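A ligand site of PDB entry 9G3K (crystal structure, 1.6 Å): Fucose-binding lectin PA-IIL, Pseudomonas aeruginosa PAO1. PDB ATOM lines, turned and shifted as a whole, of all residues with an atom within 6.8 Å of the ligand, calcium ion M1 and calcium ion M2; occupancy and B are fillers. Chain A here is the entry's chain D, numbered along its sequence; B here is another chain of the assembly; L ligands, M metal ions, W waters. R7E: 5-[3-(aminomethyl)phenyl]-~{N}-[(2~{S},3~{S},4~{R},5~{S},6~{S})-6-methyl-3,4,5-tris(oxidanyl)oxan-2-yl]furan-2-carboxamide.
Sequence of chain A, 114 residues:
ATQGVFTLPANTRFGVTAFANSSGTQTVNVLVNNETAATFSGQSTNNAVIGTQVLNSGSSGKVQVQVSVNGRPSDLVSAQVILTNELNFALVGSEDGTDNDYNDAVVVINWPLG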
ATOM      1  N   ALA A  20      -4.540  -4.728  -3.936  1.00  0.00           N
ATOM      2  CA  ALA A  20      -4.359  -6.095  -4.403  1.00  0.00           C
ATOM      3  C   ALA A  20      -3.052  -6.733  -3.948  1.00  0.00           C
ATOM      4  O   ALA A  20      -1.985  -6.117  -3.852  1.00  0.00           O
ATOM      5  CB  ALA A  20      -4.452  -6.111  -5.896  1.00  0.00           C
ATOM      6  N   ASN A  21      -3.125  -8.024  -3.646  1.00  0.00           N
ATOM      7  CA  ASN A  21      -1.989  -8.838  -3.260  1.00  0.00           C
ATOM      8  C   ASN A  21      -2.167 -10.272  -3.723  1.00  0.00           C
ATOM      9  O   ASN A  21      -2.426 -11.178  -2.930  1.00  0.00           O
ATOM     10  CB  ASN A  21      -1.821  -8.847  -1.749  1.00  0.00           C
ATOM     11  CG  ASN A  21      -1.423  -7.530  -1.144  1.00  0.00           C
ATOM     12  OD1 ASN A  21      -0.266  -7.153  -1.182  1.00  0.00           O
ATOM     13  ND2 ASN A  21      -2.372  -6.826  -0.554  1.00  0.00           N
ATOM     14  N   SER A  22      -2.097 -10.440  -5.022  1.00  0.00           N
ATOM     15  CA  SER A  22      -2.377 -11.714  -5.681  1.00  0.00           C
ATOM     16  C   SER A  22      -1.791 -11.681  -7.078  1.00  0.00           C
ATOM     17  O   SER A  22      -1.725 -10.643  -7.699  1.00  0.00           O
ATOM     18  CB  SER A  22      -3.883 -11.926  -5.751  1.00  0.00           C
ATOM     19  OG  SER A  22      -4.194 -13.095  -6.495  1.00  0.00           O
ATOM     20  N   SER A  23      -1.442 -12.884  -7.543  1.00  0.00           N
ATOM     21  CA  SER A  23      -1.022 -12.957  -8.946  1.00  0.00           C
ATOM     22  C   SER A  23      -2.174 -12.848  -9.935  1.00  0.00           C
ATOM     23  O   SER A  23      -1.890 -12.673 -11.130  1.00  0.00           O
ATOM     24  CB  SER A  23      -0.222 -14.217  -9.151  1.00  0.00           C
ATOM     25  OG  SER A  23      -1.009 -15.379  -8.874  1.00  0.00           O
ATOM     26  N   GLY A  24      -3.421 -12.931  -9.519  1.00  0.00           N
ATOM     27  CA  GLY A  24      -4.501 -12.768 -10.488  1.00  0.00           C
ATOM     28  C   GLY A  24      -5.128 -11.382 -10.396  1.00  0.00           C
ATOM     29  O   GLY A  24      -5.156 -10.802  -9.318  1.00  0.00           O
ATOM     30  N   THR A  25      -5.591 -10.837 -11.512  1.00  0.00           N
ATOM     31  CA  THR A  25      -6.335  -9.572 -11.512  1.00  0.00           C
ATOM     32  C   THR A  25      -7.537  -9.734 -10.594  1.00  0.00           C
ATOM     33  O   THR A  25      -8.286 -10.682 -10.740  1.00  0.00           O
ATOM     34  CB  THR A  25      -6.747  -9.194 -12.945  1.00  0.00           C
ATOM     35  OG1 THR A  25      -5.539  -8.931 -13.646  1.00  0.00           O
ATOM     36  CG2 THR A  25      -7.680  -8.007 -12.952  1.00  0.00           C
ATOM     37  N   GLN A  26      -7.759  -8.754  -9.697  1.00  0.00           N
ATOM     38  CA  GLN A  26      -8.927  -8.694  -8.812  1.00  0.00           C
ATOM     39  C   GLN A  26      -9.988  -7.790  -9.399  1.00  0.00           C
ATOM     40  O   GLN A  26      -9.673  -6.776  -9.948  1.00  0.00           O
ATOM     41  CB  GLN A  26      -8.485  -8.120  -7.471  1.00  0.00           C
ATOM     42  CG  GLN A  26      -7.342  -8.893  -6.843  1.00  0.00           C
ATOM     43  CD  GLN A  26      -7.752 -10.284  -6.383  1.00  0.00           C
ATOM     44  OE1 GLN A  26      -8.724 -10.453  -5.633  1.00  0.00           O
ATOM     45  NE2 GLN A  26      -7.028 -11.296  -6.857  1.00  0.00           N
ATOM     46  N   SER A  44      -1.771  -6.745  -8.510  1.00  0.00           N
ATOM     47  CA  SER A  44      -0.538  -6.431  -7.835  1.00  0.00           C
ATOM     48  C   SER A  44      -0.246  -7.543  -6.844  1.00  0.00           C
ATOM     49  O   SER A  44      -1.196  -8.021  -6.241  1.00  0.00           O
ATOM     50  CB  SER A  44      -0.708  -5.129  -7.067  1.00  0.00           C
ATOM     51  OG  SER A  44       0.522  -4.717  -6.429  1.00  0.00           O
ATOM     52  N   THR A  45       1.052  -7.830  -6.599  1.00  0.00           N
ATOM     53  CA  THR A  45       1.451  -8.614  -5.448  1.00  0.00           C
ATOM     54  C   THR A  45       2.155  -7.718  -4.435  1.00  0.00           C
ATOM     55  O   THR A  45       2.802  -8.227  -3.530  1.00  0.00           O
ATOM     56  CB  THR A  45       2.307  -9.820  -5.841  1.00  0.00           C
ATOM     57  OG1 THR A  45       3.375  -9.381  -6.681  1.00  0.00           O
ATOM     58  CG2 THR A  45       1.460 -10.850  -6.551  1.00  0.00           C
ATOM     59  N   VAL A  69     -12.470 -13.114  -9.065  1.00  0.00           N
ATOM     60  CA  VAL A  69     -11.242 -13.266  -9.810  1.00  0.00           C
ATOM     61  C   VAL A  69     -11.569 -14.137 -10.985  1.00  0.00           C
ATOM     62  O   VAL A  69     -12.083 -15.245 -10.832  1.00  0.00           O
ATOM     63  CB  VAL A  69     -10.084 -13.832  -8.934  1.00  0.00           C
ATOM     64  CG1 VAL A  69      -8.797 -13.944  -9.764  1.00  0.00           C
ATOM     65  CG2 VAL A  69      -9.829 -12.995  -7.724  1.00  0.00           C
ATOM     66  N   ASN A  70     -11.242 -13.655 -12.179  1.00  0.00           N
ATOM     67  CA  ASN A  70     -11.393 -14.419 -13.403  1.00  0.00           C
ATOM     68  C   ASN A  70     -12.793 -15.006 -13.400  1.00  0.00           C
ATOM     69  O   ASN A  70     -12.952 -16.173 -13.746  1.00  0.00           O
ATOM     70  CB  ASN A  70     -10.319 -15.514 -13.586  1.00  0.00           C
ATOM     71  CG  ASN A  70     -10.343 -16.010 -14.956  1.00  0.00           C
ATOM     72  OD1 ASN A  70     -10.456 -15.162 -15.854  1.00  0.00           O
ATOM     73  ND2 ASN A  70     -10.234 -17.343 -15.129  1.00  0.00           N
ATOM     74  N   SER A  94     -10.191 -10.829   1.289  1.00  0.00           N
ATOM     75  CA  SER A  94     -10.739 -11.793   0.367  1.00  0.00           C
ATOM     76  C   SER A  94      -9.645 -12.781  -0.002  1.00  0.00           C
ATOM     77  O   SER A  94      -8.456 -12.441  -0.073  1.00  0.00           O
ATOM     78  CB  SER A  94     -11.265 -11.103  -0.882  1.00  0.00           C
ATOM     79  OG  SER A  94     -10.239 -10.492  -1.636  1.00  0.00           O
ATOM     80  N   GLU A  95     -10.076 -14.031  -0.258  1.00  0.00           N
ATOM     81  CA  GLU A  95      -9.160 -15.139  -0.551  1.00  0.00           C
ATOM     82  C   GLU A  95      -9.584 -15.778  -1.859  1.00  0.00           C
ATOM     83  O   GLU A  95     -10.746 -16.207  -2.019  1.00  0.00           O
ATOM     84  CB  GLU A  95      -9.126 -16.152   0.567  1.00  0.00           C
ATOM     85  CG  GLU A  95      -8.279 -17.364   0.285  1.00  0.00           C
ATOM     86  CD  GLU A  95      -6.866 -16.961  -0.049  1.00  0.00           C
ATOM     87  OE1 GLU A  95      -6.241 -16.207   0.778  1.00  0.00           O
ATOM     88  OE2 GLU A  95      -6.311 -17.444  -1.058  1.00  0.00           O
ATOM     89  N   ASP A  96      -8.624 -15.861  -2.788  1.00  0.00           N
ATOM     90  CA  ASP A  96      -8.921 -16.387  -4.131  1.00  0.00           C
ATOM     91  C   ASP A  96      -8.210 -17.717  -4.360  1.00  0.00           C
ATOM     92  O   ASP A  96      -8.235 -18.232  -5.501  1.00  0.00           O
ATOM     93  CB  ASP A  96      -8.484 -15.395  -5.191  1.00  0.00           C
ATOM     94  CG  ASP A  96      -6.987 -15.088  -5.269  1.00  0.00           C
ATOM     95  OD1 ASP A  96      -6.212 -15.877  -4.740  1.00  0.00           O
ATOM     96  OD2 ASP A  96      -6.624 -14.075  -5.887  1.00  0.00           O
ATOM     97  N   GLY A  97      -7.533 -18.232  -3.360  1.00  0.00           N
ATOM     98  CA  GLY A  97      -6.670 -19.402  -3.547  1.00  0.00           C
ATOM     99  C   GLY A  97      -6.618 -20.301  -2.321  1.00  0.00           C
ATOM    100  O   GLY A  97      -7.638 -20.567  -1.701  1.00  0.00           O
ATOM    101  N   THR A  98      -5.389 -20.796  -2.056  1.00  0.00           N
ATOM    102  CA  THR A  98      -5.165 -21.872  -1.087  1.00  0.00           C
ATOM    103  C   THR A  98      -4.436 -21.467   0.187  1.00  0.00           C
ATOM    104  O   THR A  98      -4.413 -22.293   1.106  1.00  0.00           O
ATOM    105  CB  THR A  98      -4.317 -22.940  -1.742  1.00  0.00           C
ATOM    106  OG1 THR A  98      -3.092 -22.419  -2.236  1.00  0.00           O
ATOM    107  CG2 THR A  98      -5.056 -23.519  -2.931  1.00  0.00           C
ATOM    108  N   ASP A  99      -3.870 -20.282   0.253  1.00  0.00           N
ATOM    109  CA  ASP A  99      -2.979 -19.953   1.347  1.00  0.00           C
ATOM    110  C   ASP A  99      -3.651 -19.292   2.561  1.00  0.00           C
ATOM    111  O   ASP A  99      -2.953 -19.069   3.566  1.00  0.00           O
ATOM    112  CB  ASP A  99      -1.800 -19.144   0.886  1.00  0.00           C
ATOM    113  CG  ASP A  99      -2.156 -17.781   0.283  1.00  0.00           C
ATOM    114  OD1 ASP A  99      -3.346 -17.557   0.047  1.00  0.00           O
ATOM    115  OD2 ASP A  99      -1.199 -17.026  -0.005  1.00  0.00           O
ATOM    116  N   ASN A 100      -4.910 -18.943   2.429  1.00  0.00           N
ATOM    117  CA  ASN A 100      -5.646 -18.314   3.503  1.00  0.00           C
ATOM    118  C   ASN A 100      -4.925 -17.099   4.049  1.00  0.00           C
ATOM    119  O   ASN A 100      -4.933 -16.840   5.246  1.00  0.00           O
ATOM    120  CB  ASN A 100      -5.991 -19.323   4.604  1.00  0.00           C
ATOM    121  CG  ASN A 100      -6.997 -20.346   4.146  1.00  0.00           C
ATOM    122  OD1 ASN A 100      -7.830 -20.032   3.288  1.00  0.00           O
ATOM    123  ND2 ASN A 100      -6.832 -21.589   4.565  1.00  0.00           N
ATOM    124  N   ASP A 101      -4.366 -16.257   3.174  1.00  0.00           N
ATOM    125  CA  ASP A 101      -3.860 -14.964   3.614  1.00  0.00           C
ATOM    126  C   ASP A 101      -4.957 -13.870   3.643  1.00  0.00           C
ATOM    127  O   ASP A 101      -4.789 -12.874   4.274  1.00  0.00           O
ATOM    128  CB  ASP A 101      -2.600 -14.559   2.896  1.00  0.00           C
ATOM    129  CG  ASP A 101      -2.709 -14.245   1.406  1.00  0.00           C
ATOM    130  OD1 ASP A 101      -3.785 -14.489   0.814  1.00  0.00           O
ATOM    131  OD2 ASP A 101      -1.637 -13.890   0.834  1.00  0.00           O
ATOM    132  N   TYR A 102      -6.074 -14.068   2.904  1.00  0.00           N
ATOM    133  CA  TYR A 102      -7.190 -13.140   2.864  1.00  0.00           C
ATOM    134  C   TYR A 102      -6.813 -11.736   2.510  1.00  0.00           C
ATOM    135  O   TYR A 102      -7.557 -10.812   2.848  1.00  0.00           O
ATOM    136  CB  TYR A 102      -8.021 -13.258   4.153  1.00  0.00           C
ATOM    137  CG  TYR A 102      -8.963 -14.455   4.102  1.00  0.00           C
ATOM    138  CD1 TYR A 102      -8.471 -15.728   4.406  1.00  0.00           C
ATOM    139  CD2 TYR A 102     -10.259 -14.343   3.630  1.00  0.00           C
ATOM    140  CE1 TYR A 102      -9.294 -16.829   4.262  1.00  0.00           C
ATOM    141  CE2 TYR A 102     -11.059 -15.453   3.446  1.00  0.00           C
ATOM    142  CZ  TYR A 102     -10.549 -16.686   3.775  1.00  0.00           C
ATOM    143  OH  TYR A 102     -11.369 -17.807   3.601  1.00  0.00           O
ATOM    144  N   ASN A 103      -5.741 -11.559   1.744  1.00  0.00           N
ATOM    145  CA  ASN A 103      -5.276 -10.219   1.389  1.00  0.00           C
ATOM    146  C   ASN A 103      -5.324 -10.031  -0.126  1.00  0.00           C
ATOM    147  O   ASN A 103      -4.799  -9.058  -0.641  1.00  0.00           O
ATOM    148  CB  ASN A 103      -3.882  -9.917   1.894  1.00  0.00           C
ATOM    149  CG  ASN A 103      -2.825 -10.660   1.121  1.00  0.00           C
ATOM    150  OD1 ASN A 103      -3.125 -11.482   0.236  1.00  0.00           O
ATOM    151  ND2 ASN A 103      -1.569 -10.399   1.399  1.00  0.00           N
ATOM    152  N   ASP A 104      -5.977 -10.937  -0.857  1.00  0.00           N
ATOM    153  CA  ASP A 104      -5.887 -10.969  -2.308  1.00  0.00           C
ATOM    154  C   ASP A 104      -6.449  -9.717  -2.939  1.00  0.00           C
ATOM    155  O   ASP A 104      -5.849  -9.104  -3.804  1.00  0.00           O
ATOM    156  CB  ASP A 104      -6.436 -12.288  -2.815  1.00  0.00           C
ATOM    157  CG  ASP A 104      -5.686 -13.510  -2.289  1.00  0.00           C
ATOM    158  OD1 ASP A 104      -4.447 -13.402  -2.039  1.00  0.00           O
ATOM    159  OD2 ASP A 104      -6.325 -14.510  -2.020  1.00  0.00           O
ATOM    160  N   ALA A 105      -7.579  -9.293  -2.412  1.00  0.00           N
ATOM    161  CA  ALA A 105      -8.043  -7.934  -2.482  1.00  0.00           C
ATOM    162  C   ALA A 105      -8.429  -7.536  -1.063  1.00  0.00           C
ATOM    163  O   ALA A 105      -9.054  -8.328  -0.358  1.00  0.00           O
ATOM    164  CB  ALA A 105      -9.217  -7.776  -3.418  1.00  0.00           C
ATOM    165  N   PRO B 112      -0.578  -9.190   6.234  1.00  0.00           N
ATOM    166  CA  PRO B 112       0.570  -9.310   5.341  1.00  0.00           C
ATOM    167  C   PRO B 112       0.281  -8.875   3.945  1.00  0.00           C
ATOM    168  O   PRO B 112      -0.827  -8.680   3.517  1.00  0.00           O
ATOM    169  CB  PRO B 112       0.789 -10.879   5.352  1.00  0.00           C
ATOM    170  CG  PRO B 112      -0.547 -11.395   5.508  1.00  0.00           C
ATOM    171  CD  PRO B 112      -1.221 -10.473   6.483  1.00  0.00           C
ATOM    172  N   LEU B 113       1.366  -8.718   3.214  1.00  0.00           N
ATOM    173  CA  LEU B 113       1.306  -8.390   1.790  1.00  0.00           C
ATOM    174  C   LEU B 113       1.635  -9.625   0.974  1.00  0.00           C
ATOM    175  O   LEU B 113       2.052 -10.665   1.488  1.00  0.00           O
ATOM    176  CB  LEU B 113       2.257  -7.246   1.449  1.00  0.00           C
ATOM    177  CG  LEU B 113       2.067  -5.947   2.206  1.00  0.00           C
ATOM    178  CD1 LEU B 113       2.935  -4.843   1.584  1.00  0.00           C
ATOM    179  CD2 LEU B 113       0.629  -5.491   2.339  1.00  0.00           C
ATOM    180  N   GLY B 114       1.459  -9.482  -0.339  1.00  0.00           N
ATOM    181  CA  GLY B 114       1.887 -10.507  -1.289  1.00  0.00           C
ATOM    182  C   GLY B 114       0.802 -11.498  -1.682  1.00  0.00           C
ATOM    183  O   GLY B 114      -0.161 -11.776  -0.920  1.00  0.00           O
ATOM    184  OXT GLY B 114       1.025 -12.132  -2.762  1.00  0.00           O
HETATM  185  N1  R7E L   1      -3.459 -16.121  -6.257  1.00  0.00           N
HETATM  186  C4  R7E L   1      -0.606 -15.054  -3.348  1.00  0.00           C
HETATM  187  C5  R7E L   1      -0.273 -15.406  -4.789  1.00  0.00           C
HETATM  188  C6  R7E L   1       0.745 -14.488  -5.401  1.00  0.00           C
HETATM  189  C7  R7E L   1      -3.414 -16.977  -7.284  1.00  0.00           C
HETATM  190  C8  R7E L   1      -4.452 -16.846  -8.277  1.00  0.00           C
HETATM  191  C10 R7E L   1      -6.128 -16.387  -9.658  1.00  0.00           C
HETATM  192  C13 R7E L   1      -5.031 -19.479 -11.429  1.00  0.00           C
HETATM  193  C15 R7E L   1      -5.973 -19.873 -13.599  1.00  0.00           C
HETATM  194  C17 R7E L   1      -6.429 -17.790 -12.438  1.00  0.00           C
HETATM  195  C1  R7E L   1      -2.481 -16.165  -5.252  1.00  0.00           C
HETATM  196  O5  R7E L   1      -1.416 -15.294  -5.644  1.00  0.00           O
HETATM  197  C3  R7E L   1      -1.837 -15.824  -2.923  1.00  0.00           C
HETATM  198  O3  R7E L   1      -2.187 -15.364  -1.628  1.00  0.00           O
HETATM  199  C2  R7E L   1      -2.981 -15.655  -3.898  1.00  0.00           C
HETATM  200  O2  R7E L   1      -4.041 -16.445  -3.369  1.00  0.00           O
HETATM  201  O4  R7E L   1      -0.897 -13.672  -3.215  1.00  0.00           O
HETATM  202  O7  R7E L   1      -2.575 -17.876  -7.387  1.00  0.00           O
HETATM  203  O8  R7E L   1      -4.377 -17.729  -9.381  1.00  0.00           O
HETATM  204  C11 R7E L   1      -5.435 -17.421 -10.191  1.00  0.00           C
HETATM  205  C9  R7E L   1      -5.474 -16.010  -8.455  1.00  0.00           C
HETATM  206  C12 R7E L   1      -5.610 -18.223 -11.394  1.00  0.00           C
HETATM  207  C16 R7E L   1      -6.584 -18.613 -13.533  1.00  0.00           C
HETATM  208  C14 R7E L   1      -5.160 -20.294 -12.554  1.00  0.00           C
HETATM  209  C18 R7E L   1      -4.534 -21.671 -12.572  1.00  0.00           C
HETATM  210  N2  R7E L   1      -3.097 -21.625 -12.927  1.00  0.00           N
HETATM  211 CA    CA M   1      -2.248 -12.903  -1.309  1.00  0.00          CA
HETATM  212 CA    CA M   2      -4.563 -15.825  -0.973  1.00  0.00          CA
HETATM  213  O   HOH W   1      -3.327 -19.197  -3.150  1.00  0.00           O
HETATM  214  O   HOH W   2      -1.603 -19.183  -9.622  1.00  0.00           O
HETATM  215  O   HOH W   3       0.611 -17.297  -7.608  1.00  0.00           O
HETATM  216  O   HOH W   4      -0.331 -19.197  -5.894  1.00  0.00           O
HETATM  217  O   HOH W   5      -3.067 -24.254 -13.806  1.00  0.00           O
HETATM  218  O   HOH W   6      -4.008 -20.225  -5.944  1.00  0.00           O
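The side-chain carboxylate of Asp 96 lies within hydrogen-bond range of a nitrogen (N1) of the ligand (3.2 Å).
The backbone NH of Ser 23 lies within hydrogen-bond range of an oxygen (O5) of the ligand (3.1 Å).
An oxygen (O5) of the ligand sits at hydrogen-bond distance from the side-chain hydroxyl (OG) of Ser 23 (3.3 Å).
The side-chain hydroxyl of Ser 22 is in hydrogen-bond range of a nitrogen (N1) of the ligand, at 3.1 Å.
ND2 of Asn 103 is in hydrogen-bond range of O of Pro 112 of chain B.
The side-chain carboxylate of Asp 104 lies close to the backbone NH of Asp 96 (2.8 Å).
OE2 of Glu 95 lies close to N of Gly 97.
The backbone NH (N) of Tyr 102 sits close to the side-chain carboxylate (OE1) of Glu 95, at 3.0 Å.
OG of Ser 22 lies within hydrogen-bond range of OD2 of Asp 96 (2.7 Å).
The side-chain amide nitrogen (NE2) of Gln 26 sits at hydrogen-bond distance from the side-chain carboxylate (OD2) of Asp 96.
The side-chain hydroxyl of Ser 22 is in hydrogen-bond range of the side-chain amide nitrogen of Gln 26, at 3.4 Å.
N of Ser 22 lies within hydrogen-bond range of O of Ser 44 (2.9 Å).
Merely in contact with the ligand: Val 69, Gly 24, Thr 45 and Gly 97.
Hydrophobic or aromatic side chains within 4 Å of the ligand: Val 69.
Within 4 Å of the ligand: Asn 21, Ser 22, Ser 23, Gly 24, Thr 45, Val 69, Glu 95, Asp 96, Gly 97, Asp 99, Asp 101, Asp 104 and Gly 114 of chain B.
Five residues have an atom within 4 Å of calcium ion M1: Asn 21, Asp 101, Asn 103, Asp 104 and Gly 114 of chain B.
The nearest printed residue that does not touch calcium ion M1 is Asp 99 (4.4 Å).
Four residues have an atom within 4 Å of calcium ion M2: Glu 95, Asp 99, Asp 101 and Asp 104.
The nearest printed residue that does not touch calcium ion M2 is Asp 96 (4.1 Å).
Calcium ion M1 is bound by OD1 of Asn 103 (2.3 Å), OD1 of Asp 104 (2.4 Å), O of Asn 21 (2.4 Å), O of Gly 114 of chain B (2.4 Å), OD2 of Asp 101 (2.4 Å), O4 of the ligand (2.5 Å) and O3 of the ligand (2.5 Å).
Slightly farther from calcium ion M1 lies the side-chain carboxylate (OD1) of Asp 101 (3.1 Å).
Calcium ion M2 is bound by the side-chain carboxylate (OD1) of Asp 99 (2.3 Å), the side-chain carboxylate (OD1) of Asp 101 (2.4 Å), the side-chain carboxylate (OE2) of Glu 95 (2.4 Å), the side-chain carboxylate (OD2) of Asp 104 (2.4 Å), the side-chain carboxylate (OE1) of Glu 95 (2.5 Å), an oxygen (O3) of the ligand (2.5 Å), an oxygen (O2) of the ligand (2.5 Å) and the side-chain carboxylate (OD1) of Asp 104 (2.6 Å).
Calcium ion M2 has eight donor atoms within binding distance.
Water W3 lies within hydrogen-bond range of the side-chain hydroxyl (OG) of Ser 23 and an oxygen (O7) of the ligand.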
